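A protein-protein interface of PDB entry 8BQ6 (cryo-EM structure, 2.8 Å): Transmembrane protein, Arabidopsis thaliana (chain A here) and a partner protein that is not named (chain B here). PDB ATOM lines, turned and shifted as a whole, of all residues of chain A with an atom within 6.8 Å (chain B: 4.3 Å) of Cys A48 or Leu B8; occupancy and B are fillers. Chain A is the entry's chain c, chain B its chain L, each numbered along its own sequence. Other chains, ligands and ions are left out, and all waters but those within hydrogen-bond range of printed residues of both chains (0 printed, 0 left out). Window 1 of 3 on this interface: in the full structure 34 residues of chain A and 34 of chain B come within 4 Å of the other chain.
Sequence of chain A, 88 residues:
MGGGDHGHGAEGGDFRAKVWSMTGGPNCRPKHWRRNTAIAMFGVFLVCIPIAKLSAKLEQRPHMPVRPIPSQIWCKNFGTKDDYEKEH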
ATOM      1  N   PHE A  42       2.824 -12.799  -5.751  1.00  0.00           N
ATOM      2  CA  PHE A  42       3.205 -13.845  -6.691  1.00  0.00           C
ATOM      3  C   PHE A  42       2.221 -15.016  -6.635  1.00  0.00           C
ATOM      4  O   PHE A  42       1.794 -15.528  -7.674  1.00  0.00           O
ATOM      5  CB  PHE A  42       4.640 -14.281  -6.359  1.00  0.00           C
ATOM      6  CG  PHE A  42       5.174 -15.391  -7.213  1.00  0.00           C
ATOM      7  CD1 PHE A  42       5.752 -15.121  -8.444  1.00  0.00           C
ATOM      8  CD2 PHE A  42       5.091 -16.709  -6.789  1.00  0.00           C
ATOM      9  CE1 PHE A  42       6.254 -16.138  -9.230  1.00  0.00           C
ATOM     10  CE2 PHE A  42       5.579 -17.737  -7.573  1.00  0.00           C
ATOM     11  CZ  PHE A  42       6.166 -17.451  -8.797  1.00  0.00           C
ATOM     12  N   GLY A  43       1.814 -15.423  -5.431  1.00  0.00           N
ATOM     13  CA  GLY A  43       0.872 -16.527  -5.311  1.00  0.00           C
ATOM     14  C   GLY A  43      -0.447 -16.261  -6.011  1.00  0.00           C
ATOM     15  O   GLY A  43      -1.005 -17.142  -6.668  1.00  0.00           O
ATOM     16  N   VAL A  44      -0.970 -15.039  -5.873  1.00  0.00           N
ATOM     17  CA  VAL A  44      -2.222 -14.695  -6.540  1.00  0.00           C
ATOM     18  C   VAL A  44      -2.035 -14.697  -8.051  1.00  0.00           C
ATOM     19  O   VAL A  44      -2.886 -15.194  -8.799  1.00  0.00           O
ATOM     20  CB  VAL A  44      -2.743 -13.337  -6.031  1.00  0.00           C
ATOM     21  CG1 VAL A  44      -3.607 -12.659  -7.086  1.00  0.00           C
ATOM     22  CG2 VAL A  44      -3.509 -13.520  -4.739  1.00  0.00           C
ATOM     23  N   PHE A  45      -0.916 -14.146  -8.524  1.00  0.00           N
ATOM     24  CA  PHE A  45      -0.649 -14.124  -9.957  1.00  0.00           C
ATOM     25  C   PHE A  45      -0.461 -15.536 -10.505  1.00  0.00           C
ATOM     26  O   PHE A  45      -0.922 -15.847 -11.609  1.00  0.00           O
ATOM     27  CB  PHE A  45       0.565 -13.232 -10.233  1.00  0.00           C
ATOM     28  CG  PHE A  45       1.249 -13.503 -11.540  1.00  0.00           C
ATOM     29  CD1 PHE A  45       2.275 -14.422 -11.619  1.00  0.00           C
ATOM     30  CD2 PHE A  45       0.879 -12.825 -12.686  1.00  0.00           C
ATOM     31  CE1 PHE A  45       2.910 -14.680 -12.810  1.00  0.00           C
ATOM     32  CE2 PHE A  45       1.512 -13.076 -13.884  1.00  0.00           C
ATOM     33  CZ  PHE A  45       2.530 -14.006 -13.945  1.00  0.00           C
ATOM     34  N   LEU A  46       0.209 -16.407  -9.745  1.00  0.00           N
ATOM     35  CA  LEU A  46       0.328 -17.809 -10.147  1.00  0.00           C
ATOM     36  C   LEU A  46      -1.015 -18.523 -10.097  1.00  0.00           C
ATOM     37  O   LEU A  46      -1.275 -19.424 -10.902  1.00  0.00           O
ATOM     38  CB  LEU A  46       1.344 -18.545  -9.270  1.00  0.00           C
ATOM     39  CG  LEU A  46       2.841 -18.358  -9.504  1.00  0.00           C
ATOM     40  CD1 LEU A  46       3.284 -19.242 -10.651  1.00  0.00           C
ATOM     41  CD2 LEU A  46       3.177 -16.936  -9.815  1.00  0.00           C
ATOM     42  N   VAL A  47      -1.866 -18.166  -9.133  1.00  0.00           N
ATOM     43  CA  VAL A  47      -3.213 -18.729  -9.081  1.00  0.00           C
ATOM     44  C   VAL A  47      -4.048 -18.228 -10.250  1.00  0.00           C
ATOM     45  O   VAL A  47      -4.866 -18.970 -10.811  1.00  0.00           O
ATOM     46  CB  VAL A  47      -3.870 -18.400  -7.726  1.00  0.00           C
ATOM     47  CG1 VAL A  47      -5.377 -18.543  -7.806  1.00  0.00           C
ATOM     48  CG2 VAL A  47      -3.318 -19.308  -6.644  1.00  0.00           C
ATOM     49  N   CYS A  48      -3.851 -16.968 -10.644  1.00  0.00           N
ATOM     50  CA  CYS A  48      -4.656 -16.372 -11.703  1.00  0.00           C
ATOM     51  C   CYS A  48      -4.393 -17.008 -13.061  1.00  0.00           C
ATOM     52  O   CYS A  48      -5.256 -16.944 -13.943  1.00  0.00           O
ATOM     53  CB  CYS A  48      -4.381 -14.871 -11.785  1.00  0.00           C
ATOM     54  SG  CYS A  48      -5.354 -13.850 -10.669  1.00  0.00           S
ATOM     55  N   ILE A  49      -3.214 -17.585 -13.268  1.00  0.00           N
ATOM     56  CA  ILE A  49      -2.851 -18.088 -14.592  1.00  0.00           C
ATOM     57  C   ILE A  49      -3.752 -19.249 -15.007  1.00  0.00           C
ATOM     58  O   ILE A  49      -4.331 -19.192 -16.100  1.00  0.00           O
ATOM     59  CB  ILE A  49      -1.360 -18.463 -14.660  1.00  0.00           C
ATOM     60  CG1 ILE A  49      -0.539 -17.251 -15.093  1.00  0.00           C
ATOM     61  CG2 ILE A  49      -1.129 -19.612 -15.627  1.00  0.00           C
ATOM     62  CD1 ILE A  49       0.917 -17.366 -14.752  1.00  0.00           C
ATOM     63  N   PRO A  50      -3.918 -20.313 -14.207  1.00  0.00           N
ATOM     64  CA  PRO A  50      -4.875 -21.354 -14.612  1.00  0.00           C
ATOM     65  C   PRO A  50      -6.299 -20.849 -14.714  1.00  0.00           C
ATOM     66  O   PRO A  50      -7.055 -21.325 -15.570  1.00  0.00           O
ATOM     67  CB  PRO A  50      -4.728 -22.419 -13.515  1.00  0.00           C
ATOM     68  CG  PRO A  50      -3.407 -22.164 -12.920  1.00  0.00           C
ATOM     69  CD  PRO A  50      -3.245 -20.684 -12.952  1.00  0.00           C
ATOM     70  N   ILE A  51      -6.686 -19.897 -13.865  1.00  0.00           N
ATOM     71  CA  ILE A  51      -8.036 -19.346 -13.932  1.00  0.00           C
ATOM     72  C   ILE A  51      -8.270 -18.684 -15.279  1.00  0.00           C
ATOM     73  O   ILE A  51      -9.302 -18.898 -15.926  1.00  0.00           O
ATOM     74  CB  ILE A  51      -8.269 -18.359 -12.775  1.00  0.00           C
ATOM     75  CG1 ILE A  51      -8.259 -19.094 -11.437  1.00  0.00           C
ATOM     76  CG2 ILE A  51      -9.577 -17.610 -12.973  1.00  0.00           C
ATOM     77  CD1 ILE A  51      -8.324 -18.176 -10.242  1.00  0.00           C
ATOM     78  N   ALA A  52      -7.310 -17.871 -15.724  1.00  0.00           N
ATOM     79  CA  ALA A  52      -7.460 -17.169 -16.993  1.00  0.00           C
ATOM     80  C   ALA A  52      -7.509 -18.143 -18.161  1.00  0.00           C
ATOM     81  O   ALA A  52      -8.292 -17.956 -19.100  1.00  0.00           O
ATOM     82  CB  ALA A  52      -6.320 -16.169 -17.174  1.00  0.00           C
ATOM     83  N   LYS A  53      -6.678 -19.186 -18.125  1.00  0.00           N
ATOM     84  CA  LYS A  53      -6.693 -20.176 -19.196  1.00  0.00           C
ATOM     85  C   LYS A  53      -8.036 -20.889 -19.264  1.00  0.00           C
ATOM     86  O   LYS A  53      -8.577 -21.117 -20.352  1.00  0.00           O
ATOM     87  CB  LYS A  53      -5.562 -21.183 -18.995  1.00  0.00           C
ATOM     88  CG  LYS A  53      -4.216 -20.682 -19.465  1.00  0.00           C
ATOM     89  CD  LYS A  53      -3.331 -21.828 -19.900  1.00  0.00           C
ATOM     90  CE  LYS A  53      -1.963 -21.330 -20.304  1.00  0.00           C
ATOM     91  NZ  LYS A  53      -0.965 -21.545 -19.221  1.00  0.00           N
ATOM     92  N   LEU B   4     -11.615 -13.950 -14.073  1.00  0.00           N
ATOM     93  CA  LEU B   4     -10.752 -13.144 -13.217  1.00  0.00           C
ATOM     94  C   LEU B   4     -11.502 -11.954 -12.642  1.00  0.00           C
ATOM     95  O   LEU B   4     -11.102 -11.396 -11.615  1.00  0.00           O
ATOM     96  CB  LEU B   4      -9.526 -12.663 -13.987  1.00  0.00           C
ATOM     97  CG  LEU B   4      -8.585 -13.713 -14.569  1.00  0.00           C
ATOM     98  CD1 LEU B   4      -8.019 -13.226 -15.887  1.00  0.00           C
ATOM     99  CD2 LEU B   4      -7.475 -14.029 -13.584  1.00  0.00           C
ATOM    100  N   ILE B   5     -12.578 -11.530 -13.301  1.00  0.00           N
ATOM    101  CA  ILE B   5     -13.359 -10.422 -12.770  1.00  0.00           C
ATOM    102  C   ILE B   5     -14.034 -10.837 -11.470  1.00  0.00           C
ATOM    103  O   ILE B   5     -13.932 -10.151 -10.446  1.00  0.00           O
ATOM    104  CB  ILE B   5     -14.383  -9.943 -13.812  1.00  0.00           C
ATOM    105  CG1 ILE B   5     -13.676  -9.154 -14.910  1.00  0.00           C
ATOM    106  CG2 ILE B   5     -15.425  -9.068 -13.156  1.00  0.00           C
ATOM    107  CD1 ILE B   5     -14.616  -8.507 -15.875  1.00  0.00           C
ATOM    108  N   VAL B   6     -14.695 -11.996 -11.487  1.00  0.00           N
ATOM    109  CA  VAL B   6     -15.470 -12.444 -10.335  1.00  0.00           C
ATOM    110  C   VAL B   6     -14.562 -12.900  -9.200  1.00  0.00           C
ATOM    111  O   VAL B   6     -14.830 -12.621  -8.026  1.00  0.00           O
ATOM    112  CB  VAL B   6     -16.443 -13.560 -10.759  1.00  0.00           C
ATOM    113  CG1 VAL B   6     -17.436 -13.856  -9.642  1.00  0.00           C
ATOM    114  CG2 VAL B   6     -17.169 -13.168 -12.032  1.00  0.00           C
ATOM    115  N   PHE B   7     -13.484 -13.615  -9.519  1.00  0.00           N
ATOM    116  CA  PHE B   7     -12.737 -14.346  -8.502  1.00  0.00           C
ATOM    117  C   PHE B   7     -11.521 -13.611  -7.961  1.00  0.00           C
ATOM    118  O   PHE B   7     -10.911 -14.091  -7.000  1.00  0.00           O
ATOM    119  CB  PHE B   7     -12.306 -15.707  -9.049  1.00  0.00           C
ATOM    120  CG  PHE B   7     -13.439 -16.668  -9.193  1.00  0.00           C
ATOM    121  CD1 PHE B   7     -14.012 -17.241  -8.073  1.00  0.00           C
ATOM    122  CD2 PHE B   7     -13.944 -16.988 -10.437  1.00  0.00           C
ATOM    123  CE1 PHE B   7     -15.061 -18.119  -8.194  1.00  0.00           C
ATOM    124  CE2 PHE B   7     -14.994 -17.869 -10.562  1.00  0.00           C
ATOM    125  CZ  PHE B   7     -15.553 -18.433  -9.439  1.00  0.00           C
ATOM    126  N   LEU B   8     -11.147 -12.480  -8.545  1.00  0.00           N
ATOM    127  CA  LEU B   8     -10.054 -11.694  -7.975  1.00  0.00           C
ATOM    128  C   LEU B   8     -10.375 -11.148  -6.590  1.00  0.00           C
ATOM    129  O   LEU B   8      -9.519 -11.261  -5.696  1.00  0.00           O
ATOM    130  CB  LEU B   8      -9.676 -10.574  -8.944  1.00  0.00           C
ATOM    131  CG  LEU B   8      -8.451 -10.859  -9.796  1.00  0.00           C
ATOM    132  CD1 LEU B   8      -8.305  -9.749 -10.804  1.00  0.00           C
ATOM    133  CD2 LEU B   8      -7.224 -10.965  -8.911  1.00  0.00           C
ATOM    134  N   PRO B   9     -11.539 -10.537  -6.338  1.00  0.00           N
ATOM    135  CA  PRO B   9     -11.845 -10.118  -4.960  1.00  0.00           C
ATOM    136  C   PRO B   9     -11.884 -11.272  -3.975  1.00  0.00           C
ATOM    137  O   PRO B   9     -11.550 -11.078  -2.800  1.00  0.00           O
ATOM    138  CB  PRO B   9     -13.215  -9.436  -5.085  1.00  0.00           C
ATOM    139  CG  PRO B   9     -13.389  -9.146  -6.514  1.00  0.00           C
ATOM    140  CD  PRO B   9     -12.605 -10.143  -7.277  1.00  0.00           C
ATOM    141  N   LEU B  10     -12.303 -12.462  -4.410  1.00  0.00           N
ATOM    142  CA  LEU B  10     -12.239 -13.631  -3.538  1.00  0.00           C
ATOM    143  C   LEU B  10     -10.799 -13.956  -3.173  1.00  0.00           C
ATOM    144  O   LEU B  10     -10.496 -14.268  -2.016  1.00  0.00           O
ATOM    145  CB  LEU B  10     -12.899 -14.828  -4.218  1.00  0.00           C
ATOM    146  CG  LEU B  10     -12.918 -16.151  -3.452  1.00  0.00           C
ATOM    147  CD1 LEU B  10     -13.504 -15.984  -2.059  1.00  0.00           C
ATOM    148  CD2 LEU B  10     -13.670 -17.207  -4.238  1.00  0.00           C
ATOM    149  N   LEU B  11      -9.898 -13.885  -4.154  1.00  0.00           N
ATOM    150  CA  LEU B  11      -8.481 -14.113  -3.898  1.00  0.00           C
ATOM    151  C   LEU B  11      -7.923 -13.058  -2.954  1.00  0.00           C
ATOM    152  O   LEU B  11      -7.118 -13.361  -2.067  1.00  0.00           O
ATOM    153  CB  LEU B  11      -7.715 -14.103  -5.217  1.00  0.00           C
ATOM    154  CG  LEU B  11      -7.937 -15.289  -6.151  1.00  0.00           C
ATOM    155  CD1 LEU B  11      -7.271 -15.006  -7.479  1.00  0.00           C
ATOM    156  CD2 LEU B  11      -7.410 -16.572  -5.543  1.00  0.00           C
ATOM    157  N   GLY B  12      -8.329 -11.802  -3.142  1.00  0.00           N
ATOM    158  CA  GLY B  12      -7.863 -10.753  -2.255  1.00  0.00           C
ATOM    159  C   GLY B  12      -8.333 -10.952  -0.828  1.00  0.00           C
ATOM    160  O   GLY B  12      -7.568 -10.763   0.121  1.00  0.00           O
ATOM    161  N   CYS B  35      -6.134  -6.407  -5.879  1.00  0.00           N
ATOM    162  CA  CYS B  35      -6.985  -7.396  -6.537  1.00  0.00           C
ATOM    163  C   CYS B  35      -8.318  -6.796  -6.965  1.00  0.00           C
ATOM    164  O   CYS B  35      -8.815  -7.085  -8.060  1.00  0.00           O
ATOM    165  CB  CYS B  35      -7.216  -8.590  -5.613  1.00  0.00           C
ATOM    166  SG  CYS B  35      -5.721  -9.488  -5.186  1.00  0.00           S
ATOM    167  N   PHE B  38      -7.562  -4.384  -9.900  1.00  0.00           N
ATOM    168  CA  PHE B  38      -7.351  -5.121 -11.143  1.00  0.00           C
ATOM    169  C   PHE B  38      -8.671  -5.600 -11.719  1.00  0.00           C
ATOM    170  O   PHE B  38      -8.892  -5.523 -12.933  1.00  0.00           O
ATOM    171  CB  PHE B  38      -6.446  -6.331 -10.939  1.00  0.00           C
ATOM    172  CG  PHE B  38      -4.998  -6.057 -11.162  1.00  0.00           C
ATOM    173  CD1 PHE B  38      -4.231  -5.455 -10.187  1.00  0.00           C
ATOM    174  CD2 PHE B  38      -4.416  -6.340 -12.380  1.00  0.00           C
ATOM    175  CE1 PHE B  38      -2.896  -5.203 -10.402  1.00  0.00           C
ATOM    176  CE2 PHE B  38      -3.087  -6.073 -12.601  1.00  0.00           C
ATOM    177  CZ  PHE B  38      -2.327  -5.507 -11.609  1.00  0.00           C
ATOM    178  N   SER B  39      -9.541  -6.135 -10.863  1.00  0.00           N
ATOM    179  CA  SER B  39     -10.862  -6.551 -11.312  1.00  0.00           C
ATOM    180  C   SER B  39     -11.654  -5.362 -11.830  1.00  0.00           C
ATOM    181  O   SER B  39     -12.482  -5.503 -12.737  1.00  0.00           O
ATOM    182  CB  SER B  39     -11.605  -7.243 -10.171  1.00  0.00           C
ATOM    183  OG  SER B  39     -13.001  -7.049 -10.295  1.00  0.00           O
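Printed residues of chain B within 4 Å of Val A47: Leu B11 (3.6 Å).
Of the printed residues of chain B, Cys A48 touches Leu B4 (3.6 Å), Leu B8 (3.9 Å) and Leu B11 (3.9 Å).
Ile A49 touches none of the printed residues of chain B.
Of the printed residues of chain B, Ala A52 touches Leu B4 (3.6 Å).
Of the printed residues of chain A, Leu B4 touches Cys A48 and Ala A52.
Leu B8 touches just one residue of chain A: Cys A48.
Of the printed residues of chain A, Leu B11 touches Val A47 (3.6 Å) and Cys A48 (3.9 Å).
The nearest printed residue of chain B that does not touch Val A47 is Leu B4 (6.2 Å).
The side-chain sulfur of Cys A48 sits close to the backbone carbonyl oxygen of Val A44 (3.4 Å).
Of the 12 printed residues of chain A, 3 touch a printed residue of chain B.
Hydrophobic or aromatic side chains of chain A that line the printed part of chain B: Val A47 and Ala A52.
Among the printed residues, 5 pairs touch across the chains.
Among the printed residues, no Asp or Glu carboxylate lies within 4 Å of a Lys or Arg side-chain nitrogen of the other chain.
Among the printed residues, merely in contact across the chains: Val A47 with Leu B11 (3.6 Å), Cys A48 with Leu B4 (3.6 Å), Cys A48 with Leu B8 (3.9 Å), Cys A48 with Leu B11 (3.9 Å) and Ala A52 with Leu B4 (3.6 Å).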
